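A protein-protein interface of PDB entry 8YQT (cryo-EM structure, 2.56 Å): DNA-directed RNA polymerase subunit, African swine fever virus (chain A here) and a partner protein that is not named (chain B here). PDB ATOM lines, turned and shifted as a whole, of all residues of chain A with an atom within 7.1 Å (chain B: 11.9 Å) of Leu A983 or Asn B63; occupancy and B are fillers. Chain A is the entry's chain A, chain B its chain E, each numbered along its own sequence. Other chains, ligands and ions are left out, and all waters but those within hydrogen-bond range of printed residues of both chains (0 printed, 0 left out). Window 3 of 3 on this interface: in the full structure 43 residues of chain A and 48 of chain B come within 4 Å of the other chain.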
ATOM      1  N   TYR A 973     -18.107  13.334 -26.790  1.00  0.00           N
ATOM      2  CA  TYR A 973     -18.784  14.432 -26.110  1.00  0.00           C
ATOM      3  C   TYR A 973     -18.162  15.783 -26.405  1.00  0.00           C
ATOM      4  O   TYR A 973     -18.752  16.805 -26.044  1.00  0.00           O
ATOM      5  CB  TYR A 973     -18.808  14.195 -24.601  1.00  0.00           C
ATOM      6  CG  TYR A 973     -19.780  13.126 -24.172  1.00  0.00           C
ATOM      7  CD1 TYR A 973     -21.137  13.262 -24.411  1.00  0.00           C
ATOM      8  CD2 TYR A 973     -19.342  11.985 -23.519  1.00  0.00           C
ATOM      9  CE1 TYR A 973     -22.029  12.293 -24.021  1.00  0.00           C
ATOM     10  CE2 TYR A 973     -20.228  11.010 -23.124  1.00  0.00           C
ATOM     11  CZ  TYR A 973     -21.570  11.170 -23.379  1.00  0.00           C
ATOM     12  OH  TYR A 973     -22.461  10.202 -22.991  1.00  0.00           O
ATOM     13  N   ASN A 978     -20.231  19.454 -22.106  1.00  0.00           N
ATOM     14  CA  ASN A 978     -19.843  18.788 -20.870  1.00  0.00           C
ATOM     15  C   ASN A 978     -21.030  18.411 -19.993  1.00  0.00           C
ATOM     16  O   ASN A 978     -20.862  17.623 -19.056  1.00  0.00           O
ATOM     17  CB  ASN A 978     -18.878  19.671 -20.074  1.00  0.00           C
ATOM     18  CG  ASN A 978     -19.511  20.969 -19.615  1.00  0.00           C
ATOM     19  OD1 ASN A 978     -20.641  21.291 -19.980  1.00  0.00           O
ATOM     20  ND2 ASN A 978     -18.782  21.723 -18.806  1.00  0.00           N
ATOM     21  N   ILE A 979     -22.216  18.964 -20.256  1.00  0.00           N
ATOM     22  CA  ILE A 979     -23.395  18.607 -19.470  1.00  0.00           C
ATOM     23  C   ILE A 979     -23.807  17.170 -19.756  1.00  0.00           C
ATOM     24  O   ILE A 979     -24.066  16.386 -18.836  1.00  0.00           O
ATOM     25  CB  ILE A 979     -24.549  19.585 -19.749  1.00  0.00           C
ATOM     26  CG1 ILE A 979     -24.115  21.028 -19.491  1.00  0.00           C
ATOM     27  CG2 ILE A 979     -25.759  19.235 -18.904  1.00  0.00           C
ATOM     28  CD1 ILE A 979     -25.003  22.049 -20.156  1.00  0.00           C
ATOM     29  N   GLN A 980     -23.876  16.804 -21.035  1.00  0.00           N
ATOM     30  CA  GLN A 980     -24.218  15.439 -21.406  1.00  0.00           C
ATOM     31  C   GLN A 980     -23.104  14.456 -21.090  1.00  0.00           C
ATOM     32  O   GLN A 980     -23.388  13.280 -20.843  1.00  0.00           O
ATOM     33  CB  GLN A 980     -24.569  15.364 -22.892  1.00  0.00           C
ATOM     34  CG  GLN A 980     -25.566  16.412 -23.346  1.00  0.00           C
ATOM     35  CD  GLN A 980     -26.887  16.324 -22.611  1.00  0.00           C
ATOM     36  OE1 GLN A 980     -27.458  15.247 -22.465  1.00  0.00           O
ATOM     37  NE2 GLN A 980     -27.377  17.461 -22.139  1.00  0.00           N
ATOM     38  N   GLU A 981     -21.849  14.906 -21.101  1.00  0.00           N
ATOM     39  CA  GLU A 981     -20.753  14.038 -20.689  1.00  0.00           C
ATOM     40  C   GLU A 981     -20.874  13.665 -19.219  1.00  0.00           C
ATOM     41  O   GLU A 981     -20.630  12.513 -18.844  1.00  0.00           O
ATOM     42  CB  GLU A 981     -19.416  14.719 -20.962  1.00  0.00           C
ATOM     43  CG  GLU A 981     -18.212  13.846 -20.675  1.00  0.00           C
ATOM     44  CD  GLU A 981     -16.908  14.589 -20.847  1.00  0.00           C
ATOM     45  OE1 GLU A 981     -16.947  15.810 -21.100  1.00  0.00           O
ATOM     46  OE2 GLU A 981     -15.842  13.951 -20.735  1.00  0.00           O
ATOM     47  N   ARG A 982     -21.241  14.628 -18.373  1.00  0.00           N
ATOM     48  CA  ARG A 982     -21.479  14.332 -16.965  1.00  0.00           C
ATOM     49  C   ARG A 982     -22.676  13.406 -16.789  1.00  0.00           C
ATOM     50  O   ARG A 982     -22.648  12.498 -15.952  1.00  0.00           O
ATOM     51  CB  ARG A 982     -21.689  15.629 -16.187  1.00  0.00           C
ATOM     52  CG  ARG A 982     -21.800  15.436 -14.689  1.00  0.00           C
ATOM     53  CD  ARG A 982     -22.136  16.736 -13.987  1.00  0.00           C
ATOM     54  NE  ARG A 982     -23.484  17.193 -14.304  1.00  0.00           N
ATOM     55  CZ  ARG A 982     -23.763  18.314 -14.954  1.00  0.00           C
ATOM     56  NH1 ARG A 982     -22.806  19.125 -15.377  1.00  0.00           N
ATOM     57  NH2 ARG A 982     -25.033  18.630 -15.186  1.00  0.00           N
ATOM     58  N   LEU A 983     -23.735  13.625 -17.568  1.00  0.00           N
ATOM     59  CA  LEU A 983     -24.935  12.806 -17.472  1.00  0.00           C
ATOM     60  C   LEU A 983     -24.795  11.465 -18.175  1.00  0.00           C
ATOM     61  O   LEU A 983     -25.625  10.578 -17.949  1.00  0.00           O
ATOM     62  CB  LEU A 983     -26.131  13.561 -18.051  1.00  0.00           C
ATOM     63  CG  LEU A 983     -26.600  14.790 -17.275  1.00  0.00           C
ATOM     64  CD1 LEU A 983     -27.700  15.504 -18.036  1.00  0.00           C
ATOM     65  CD2 LEU A 983     -27.067  14.393 -15.890  1.00  0.00           C
ATOM     66  N   GLN A 984     -23.774  11.303 -19.019  1.00  0.00           N
ATOM     67  CA  GLN A 984     -23.514  10.051 -19.732  1.00  0.00           C
ATOM     68  C   GLN A 984     -24.711   9.619 -20.573  1.00  0.00           C
ATOM     69  O   GLN A 984     -25.091   8.448 -20.592  1.00  0.00           O
ATOM     70  CB  GLN A 984     -23.101   8.940 -18.766  1.00  0.00           C
ATOM     71  CG  GLN A 984     -21.774   9.194 -18.080  1.00  0.00           C
ATOM     72  CD  GLN A 984     -20.615   9.205 -19.052  1.00  0.00           C
ATOM     73  OE1 GLN A 984     -20.491   8.321 -19.897  1.00  0.00           O
ATOM     74  NE2 GLN A 984     -19.766  10.218 -18.947  1.00  0.00           N
ATOM     75  N   THR A 985     -25.309  10.571 -21.277  1.00  0.00           N
ATOM     76  CA  THR A 985     -26.405  10.270 -22.179  1.00  0.00           C
ATOM     77  C   THR A 985     -25.884   9.561 -23.426  1.00  0.00           C
ATOM     78  O   THR A 985     -24.699   9.652 -23.753  1.00  0.00           O
ATOM     79  CB  THR A 985     -27.136  11.552 -22.562  1.00  0.00           C
ATOM     80  OG1 THR A 985     -26.232  12.439 -23.228  1.00  0.00           O
ATOM     81  CG2 THR A 985     -27.683  12.233 -21.323  1.00  0.00           C
ATOM     82  N   PRO A 986     -26.747   8.828 -24.133  1.00  0.00           N
ATOM     83  CA  PRO A 986     -26.294   8.122 -25.336  1.00  0.00           C
ATOM     84  C   PRO A 986     -25.753   9.074 -26.391  1.00  0.00           C
ATOM     85  O   PRO A 986     -26.187  10.220 -26.516  1.00  0.00           O
ATOM     86  CB  PRO A 986     -27.558   7.405 -25.825  1.00  0.00           C
ATOM     87  CG  PRO A 986     -28.686   8.076 -25.122  1.00  0.00           C
ATOM     88  CD  PRO A 986     -28.135   8.477 -23.800  1.00  0.00           C
ATOM     89  N   ILE B  59     -38.033  27.115 -23.919  1.00  0.00           N
ATOM     90  CA  ILE B  59     -36.644  27.099 -23.482  1.00  0.00           C
ATOM     91  C   ILE B  59     -36.316  25.694 -22.999  1.00  0.00           C
ATOM     92  O   ILE B  59     -36.953  25.181 -22.073  1.00  0.00           O
ATOM     93  CB  ILE B  59     -36.400  28.139 -22.380  1.00  0.00           C
ATOM     94  CG1 ILE B  59     -36.682  29.542 -22.913  1.00  0.00           C
ATOM     95  CG2 ILE B  59     -34.981  28.049 -21.866  1.00  0.00           C
ATOM     96  CD1 ILE B  59     -36.724  30.601 -21.847  1.00  0.00           C
ATOM     97  N   ILE B  60     -35.336  25.067 -23.635  1.00  0.00           N
ATOM     98  CA  ILE B  60     -34.927  23.713 -23.247  1.00  0.00           C
ATOM     99  C   ILE B  60     -34.307  23.761 -21.855  1.00  0.00           C
ATOM    100  O   ILE B  60     -33.475  24.643 -21.585  1.00  0.00           O
ATOM    101  CB  ILE B  60     -33.944  23.142 -24.270  1.00  0.00           C
ATOM    102  CG1 ILE B  60     -34.636  22.935 -25.615  1.00  0.00           C
ATOM    103  CG2 ILE B  60     -33.350  21.836 -23.783  1.00  0.00           C
ATOM    104  CD1 ILE B  60     -33.692  22.532 -26.717  1.00  0.00           C
ATOM    105  N   PRO B  61     -34.675  22.858 -20.946  1.00  0.00           N
ATOM    106  CA  PRO B  61     -34.059  22.862 -19.616  1.00  0.00           C
ATOM    107  C   PRO B  61     -32.553  22.677 -19.702  1.00  0.00           C
ATOM    108  O   PRO B  61     -32.039  21.980 -20.580  1.00  0.00           O
ATOM    109  CB  PRO B  61     -34.735  21.684 -18.904  1.00  0.00           C
ATOM    110  CG  PRO B  61     -35.354  20.869 -19.989  1.00  0.00           C
ATOM    111  CD  PRO B  61     -35.723  21.834 -21.063  1.00  0.00           C
ATOM    112  N   ASP B  62     -31.845  23.320 -18.770  1.00  0.00           N
ATOM    113  CA  ASP B  62     -30.391  23.405 -18.832  1.00  0.00           C
ATOM    114  C   ASP B  62     -29.712  22.041 -18.862  1.00  0.00           C
ATOM    115  O   ASP B  62     -28.594  21.936 -19.373  1.00  0.00           O
ATOM    116  CB  ASP B  62     -29.861  24.215 -17.649  1.00  0.00           C
ATOM    117  CG  ASP B  62     -30.152  25.697 -17.778  1.00  0.00           C
ATOM    118  OD1 ASP B  62     -30.396  26.163 -18.910  1.00  0.00           O
ATOM    119  OD2 ASP B  62     -30.128  26.401 -16.748  1.00  0.00           O
ATOM    120  N   ASN B  63     -30.353  21.001 -18.337  1.00  0.00           N
ATOM    121  CA  ASN B  63     -29.772  19.668 -18.312  1.00  0.00           C
ATOM    122  C   ASN B  63     -30.085  18.862 -19.567  1.00  0.00           C
ATOM    123  O   ASN B  63     -29.712  17.690 -19.646  1.00  0.00           O
ATOM    124  CB  ASN B  63     -30.249  18.909 -17.075  1.00  0.00           C
ATOM    125  CG  ASN B  63     -29.186  18.824 -16.001  1.00  0.00           C
ATOM    126  OD1 ASN B  63     -28.348  19.717 -15.869  1.00  0.00           O
ATOM    127  ND2 ASN B  63     -29.210  17.743 -15.230  1.00  0.00           N
ATOM    128  N   GLU B  64     -30.762  19.462 -20.543  1.00  0.00           N
ATOM    129  CA  GLU B  64     -31.081  18.796 -21.798  1.00  0.00           C
ATOM    130  C   GLU B  64     -30.484  19.513 -22.999  1.00  0.00           C
ATOM    131  O   GLU B  64     -30.821  19.177 -24.139  1.00  0.00           O
ATOM    132  CB  GLU B  64     -32.597  18.676 -21.963  1.00  0.00           C
ATOM    133  CG  GLU B  64     -33.280  17.955 -20.823  1.00  0.00           C
ATOM    134  CD  GLU B  64     -34.718  17.606 -21.137  1.00  0.00           C
ATOM    135  OE1 GLU B  64     -35.292  18.225 -22.057  1.00  0.00           O
ATOM    136  OE2 GLU B  64     -35.277  16.716 -20.463  1.00  0.00           O
ATOM    137  N   ARG B  65     -29.613  20.491 -22.775  1.00  0.00           N
ATOM    138  CA  ARG B  65     -29.004  21.236 -23.864  1.00  0.00           C
ATOM    139  C   ARG B  65     -27.980  20.377 -24.593  1.00  0.00           C
ATOM    140  O   ARG B  65     -27.219  19.628 -23.974  1.00  0.00           O
ATOM    141  CB  ARG B  65     -28.353  22.510 -23.332  1.00  0.00           C
ATOM    142  CG  ARG B  65     -29.357  23.530 -22.835  1.00  0.00           C
ATOM    143  CD  ARG B  65     -28.687  24.773 -22.293  1.00  0.00           C
ATOM    144  NE  ARG B  65     -27.997  24.511 -21.038  1.00  0.00           N
ATOM    145  CZ  ARG B  65     -27.314  25.419 -20.357  1.00  0.00           C
ATOM    146  NH1 ARG B  65     -27.228  26.671 -20.770  1.00  0.00           N
ATOM    147  NH2 ARG B  65     -26.703  25.061 -19.233  1.00  0.00           N
ATOM    148  N   ILE B  66     -27.966  20.492 -25.919  1.00  0.00           N
ATOM    149  CA  ILE B  66     -27.169  19.620 -26.775  1.00  0.00           C
ATOM    150  C   ILE B  66     -26.027  20.404 -27.412  1.00  0.00           C
ATOM    151  O   ILE B  66     -24.993  19.832 -27.769  1.00  0.00           O
ATOM    152  CB  ILE B  66     -28.070  18.942 -27.829  1.00  0.00           C
ATOM    153  CG1 ILE B  66     -28.201  17.446 -27.539  1.00  0.00           C
ATOM    154  CG2 ILE B  66     -27.586  19.195 -29.253  1.00  0.00           C
ATOM    155  CD1 ILE B  66     -28.484  17.123 -26.097  1.00  0.00           C
ATOM    156  N   THR B  67     -26.187  21.718 -27.529  1.00  0.00           N
ATOM    157  CA  THR B  67     -25.136  22.538 -28.104  1.00  0.00           C
ATOM    158  C   THR B  67     -23.978  22.689 -27.119  1.00  0.00           C
ATOM    159  O   THR B  67     -24.083  22.360 -25.935  1.00  0.00           O
ATOM    160  CB  THR B  67     -25.683  23.904 -28.512  1.00  0.00           C
ATOM    161  OG1 THR B  67     -26.311  24.526 -27.387  1.00  0.00           O
ATOM    162  CG2 THR B  67     -26.691  23.756 -29.627  1.00  0.00           C
ATOM    163  N   SER B  68     -22.856  23.191 -27.624  1.00  0.00           N
ATOM    164  CA  SER B  68     -21.624  23.219 -26.852  1.00  0.00           C
ATOM    165  C   SER B  68     -21.659  24.294 -25.775  1.00  0.00           C
ATOM    166  O   SER B  68     -22.350  25.308 -25.895  1.00  0.00           O
ATOM    167  CB  SER B  68     -20.421  23.447 -27.767  1.00  0.00           C
ATOM    168  OG  SER B  68     -20.445  24.740 -28.334  1.00  0.00           O
ATOM    169  N   ASN B  69     -20.897  24.056 -24.711  1.00  0.00           N
ATOM    170  CA  ASN B  69     -20.735  25.012 -23.627  1.00  0.00           C
ATOM    171  C   ASN B  69     -19.622  26.009 -23.890  1.00  0.00           C
ATOM    172  O   ASN B  69     -19.345  26.847 -23.031  1.00  0.00           O
ATOM    173  CB  ASN B  69     -20.460  24.286 -22.310  1.00  0.00           C
ATOM    174  CG  ASN B  69     -19.203  23.452 -22.362  1.00  0.00           C
ATOM    175  OD1 ASN B  69     -18.870  22.879 -23.393  1.00  0.00           O
ATOM    176  ND2 ASN B  69     -18.476  23.412 -21.257  1.00  0.00           N
ATOM    177  N   VAL B 133     -35.673  26.867 -28.299  1.00  0.00           N
ATOM    178  CA  VAL B 133     -34.384  27.538 -28.260  1.00  0.00           C
ATOM    179  C   VAL B 133     -33.580  27.001 -27.084  1.00  0.00           C
ATOM    180  O   VAL B 133     -34.083  26.260 -26.241  1.00  0.00           O
ATOM    181  CB  VAL B 133     -34.522  29.069 -28.144  1.00  0.00           C
ATOM    182  CG1 VAL B 133     -35.293  29.632 -29.320  1.00  0.00           C
ATOM    183  CG2 VAL B 133     -35.188  29.435 -26.830  1.00  0.00           C
ATOM    184  N   GLU B 134     -32.308  27.389 -27.043  1.00  0.00           N
ATOM    185  CA  GLU B 134     -31.427  27.119 -25.915  1.00  0.00           C
ATOM    186  C   GLU B 134     -30.837  28.433 -25.435  1.00  0.00           C
ATOM    187  O   GLU B 134     -30.349  29.227 -26.243  1.00  0.00           O
ATOM    188  CB  GLU B 134     -30.305  26.152 -26.289  1.00  0.00           C
ATOM    189  CG  GLU B 134     -30.758  24.738 -26.564  1.00  0.00           C
ATOM    190  CD  GLU B 134     -29.599  23.783 -26.728  1.00  0.00           C
ATOM    191  OE1 GLU B 134     -28.442  24.237 -26.635  1.00  0.00           O
ATOM    192  OE2 GLU B 134     -29.842  22.581 -26.954  1.00  0.00           O
ATOM    193  N   ILE B 135     -30.878  28.658 -24.127  1.00  0.00           N
ATOM    194  CA  ILE B 135     -30.310  29.854 -23.518  1.00  0.00           C
ATOM    195  C   ILE B 135     -29.004  29.470 -22.842  1.00  0.00           C
ATOM    196  O   ILE B 135     -28.960  28.525 -22.046  1.00  0.00           O
ATOM    197  CB  ILE B 135     -31.285  30.493 -22.514  1.00  0.00           C
ATOM    198  CG1 ILE B 135     -32.637  30.754 -23.172  1.00  0.00           C
ATOM    199  CG2 ILE B 135     -30.717  31.790 -21.978  1.00  0.00           C
ATOM    200  CD1 ILE B 135     -32.578  31.739 -24.302  1.00  0.00           C
ATOM    201  N   TRP B 136     -27.938  30.197 -23.163  1.00  0.00           N
ATOM    202  CA  TRP B 136     -26.612  29.930 -22.626  1.00  0.00           C
ATOM    203  C   TRP B 136     -26.085  31.178 -21.942  1.00  0.00           C
ATOM    204  O   TRP B 136     -26.231  32.286 -22.465  1.00  0.00           O
ATOM    205  CB  TRP B 136     -25.648  29.482 -23.726  1.00  0.00           C
ATOM    206  CG  TRP B 136     -25.817  28.052 -24.112  1.00  0.00           C
ATOM    207  CD1 TRP B 136     -26.586  27.563 -25.119  1.00  0.00           C
ATOM    208  CD2 TRP B 136     -25.209  26.919 -23.483  1.00  0.00           C
ATOM    209  NE1 TRP B 136     -26.496  26.196 -25.163  1.00  0.00           N
ATOM    210  CE2 TRP B 136     -25.656  25.776 -24.167  1.00  0.00           C
ATOM    211  CE3 TRP B 136     -24.331  26.762 -22.409  1.00  0.00           C
ATOM    212  CZ2 TRP B 136     -25.252  24.494 -23.817  1.00  0.00           C
ATOM    213  CZ3 TRP B 136     -23.936  25.491 -22.062  1.00  0.00           C
ATOM    214  CH2 TRP B 136     -24.394  24.374 -22.763  1.00  0.00           C
ATOM    215  N   ASN B 137     -25.469  30.992 -20.779  1.00  0.00           N
ATOM    216  CA  ASN B 137     -24.895  32.096 -20.025  1.00  0.00           C
ATOM    217  C   ASN B 137     -23.415  32.203 -20.364  1.00  0.00           C
ATOM    218  O   ASN B 137     -22.641  31.313 -19.985  1.00  0.00           O
ATOM    219  CB  ASN B 137     -25.087  31.868 -18.534  1.00  0.00           C
ATOM    220  CG  ASN B 137     -24.710  33.071 -17.707  1.00  0.00           C
ATOM    221  OD1 ASN B 137     -24.408  34.135 -18.237  1.00  0.00           O
ATOM    222  ND2 ASN B 137     -24.720  32.904 -16.394  1.00  0.00           N
ATOM    223  N   GLU B 140     -20.733  31.507 -17.781  1.00  0.00           N
ATOM    224  CA  GLU B 140     -20.487  30.129 -17.376  1.00  0.00           C
ATOM    225  C   GLU B 140     -19.958  29.288 -18.531  1.00  0.00           C
ATOM    226  O   GLU B 140     -19.943  28.057 -18.443  1.00  0.00           O
ATOM    227  CB  GLU B 140     -21.762  29.502 -16.817  1.00  0.00           C
ATOM    228  CG  GLU B 140     -22.397  30.273 -15.687  1.00  0.00           C
ATOM    229  CD  GLU B 140     -23.604  29.563 -15.123  1.00  0.00           C
ATOM    230  OE1 GLU B 140     -24.733  30.057 -15.324  1.00  0.00           O
ATOM    231  OE2 GLU B 140     -23.427  28.509 -14.479  1.00  0.00           O
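The side-chain carboxylate of Asp B62 lies within salt-bridge range of the guanidinium group of Arg B65, at 3.6 Å.
OE1 of Gln A980 lies within hydrogen-bond range of OG1 of Thr A985 (3.2 Å).
The backbone NH of Ile B66 sits at hydrogen-bond distance from the side-chain carboxylate of Glu B134.
NH1 of Arg B65 sits at hydrogen-bond distance from O of Ile B135.
OE1 of Glu B134 is in hydrogen-bond range of NE1 of Trp B136, at 3.1 Å.
NE1 of Trp B136 is in hydrogen-bond range of OG1 of Thr B67, at 2.8 Å.
Among the printed residues, pairs that only touch across the chains: Leu A983 with Asn B63 (3.4 Å), Ile A979 with Trp B136 (3.5 Å), Arg A982 with Asn B63 (3.6 Å), Ile A979 with Arg B65 (3.6 Å), Ile A979 with Asp B62 (3.7 Å), Gln A980 with Glu B64 (3.8 Å) and Gln A980 with Ile B66 (3.9 Å).
Leu A983 touches just one residue of chain B: Asn B63 (3.4 Å).
Gln A980 touches just these residues of chain B: Asn B63, Glu B64, Arg B65 and Ile B66.
No residue of chain B comes within 4 Å of Gln A984.
No residue of chain B comes within 4 Å of Thr A985.
Of the printed residues of chain A, Arg B65 touches Ile A979 and Gln A980.
Printed residues of chain A within 4 Å of Glu B64: Gln A980 (3.8 Å).
Of the printed residues of chain A, Asn B69 touches Asn A978 (3.0 Å).
Printed residues of chain A within 4 Å of Asp B62: Ile A979 (3.7 Å).
Of the printed residues of chain A, Ile B66 touches Gln A980 (3.9 Å).
Ile B60 touches none of the printed residues of chain A.
The nearest printed residue of chain A that does not touch Asn B63 is Ile A979 (4.02 Å).
ND2 of Asn A978 lies close to ND2 of Asn B69 (3.0 Å).
O of Asn B63 sits at hydrogen-bond distance from NE2 of Gln A980 (3.4 Å).
The side-chain amide nitrogen (NE2) of Gln A980 lies within hydrogen-bond range of the backbone carbonyl oxygen (O) of Arg B65 (2.8 Å).
Printed residues of chain B that touch a printed residue of chain A: Asp B62, Asn B63, Glu B64, Arg B65, Ile B66, Asn B69 and Trp B136.
Hydrophobic or aromatic side chains of chain B within 4 Å of the printed part of chain A: Ile B66 and Trp B136.
Hydrophobic or aromatic side chains of chain A that line the printed part of chain B: Ile A979 and Leu A983.
Among the printed residues, 10 pairs touch across the chains.
Among the printed residues, no Asp or Glu carboxylate lies within 4 Å of a Lys or Arg side-chain nitrogen of the other chain.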
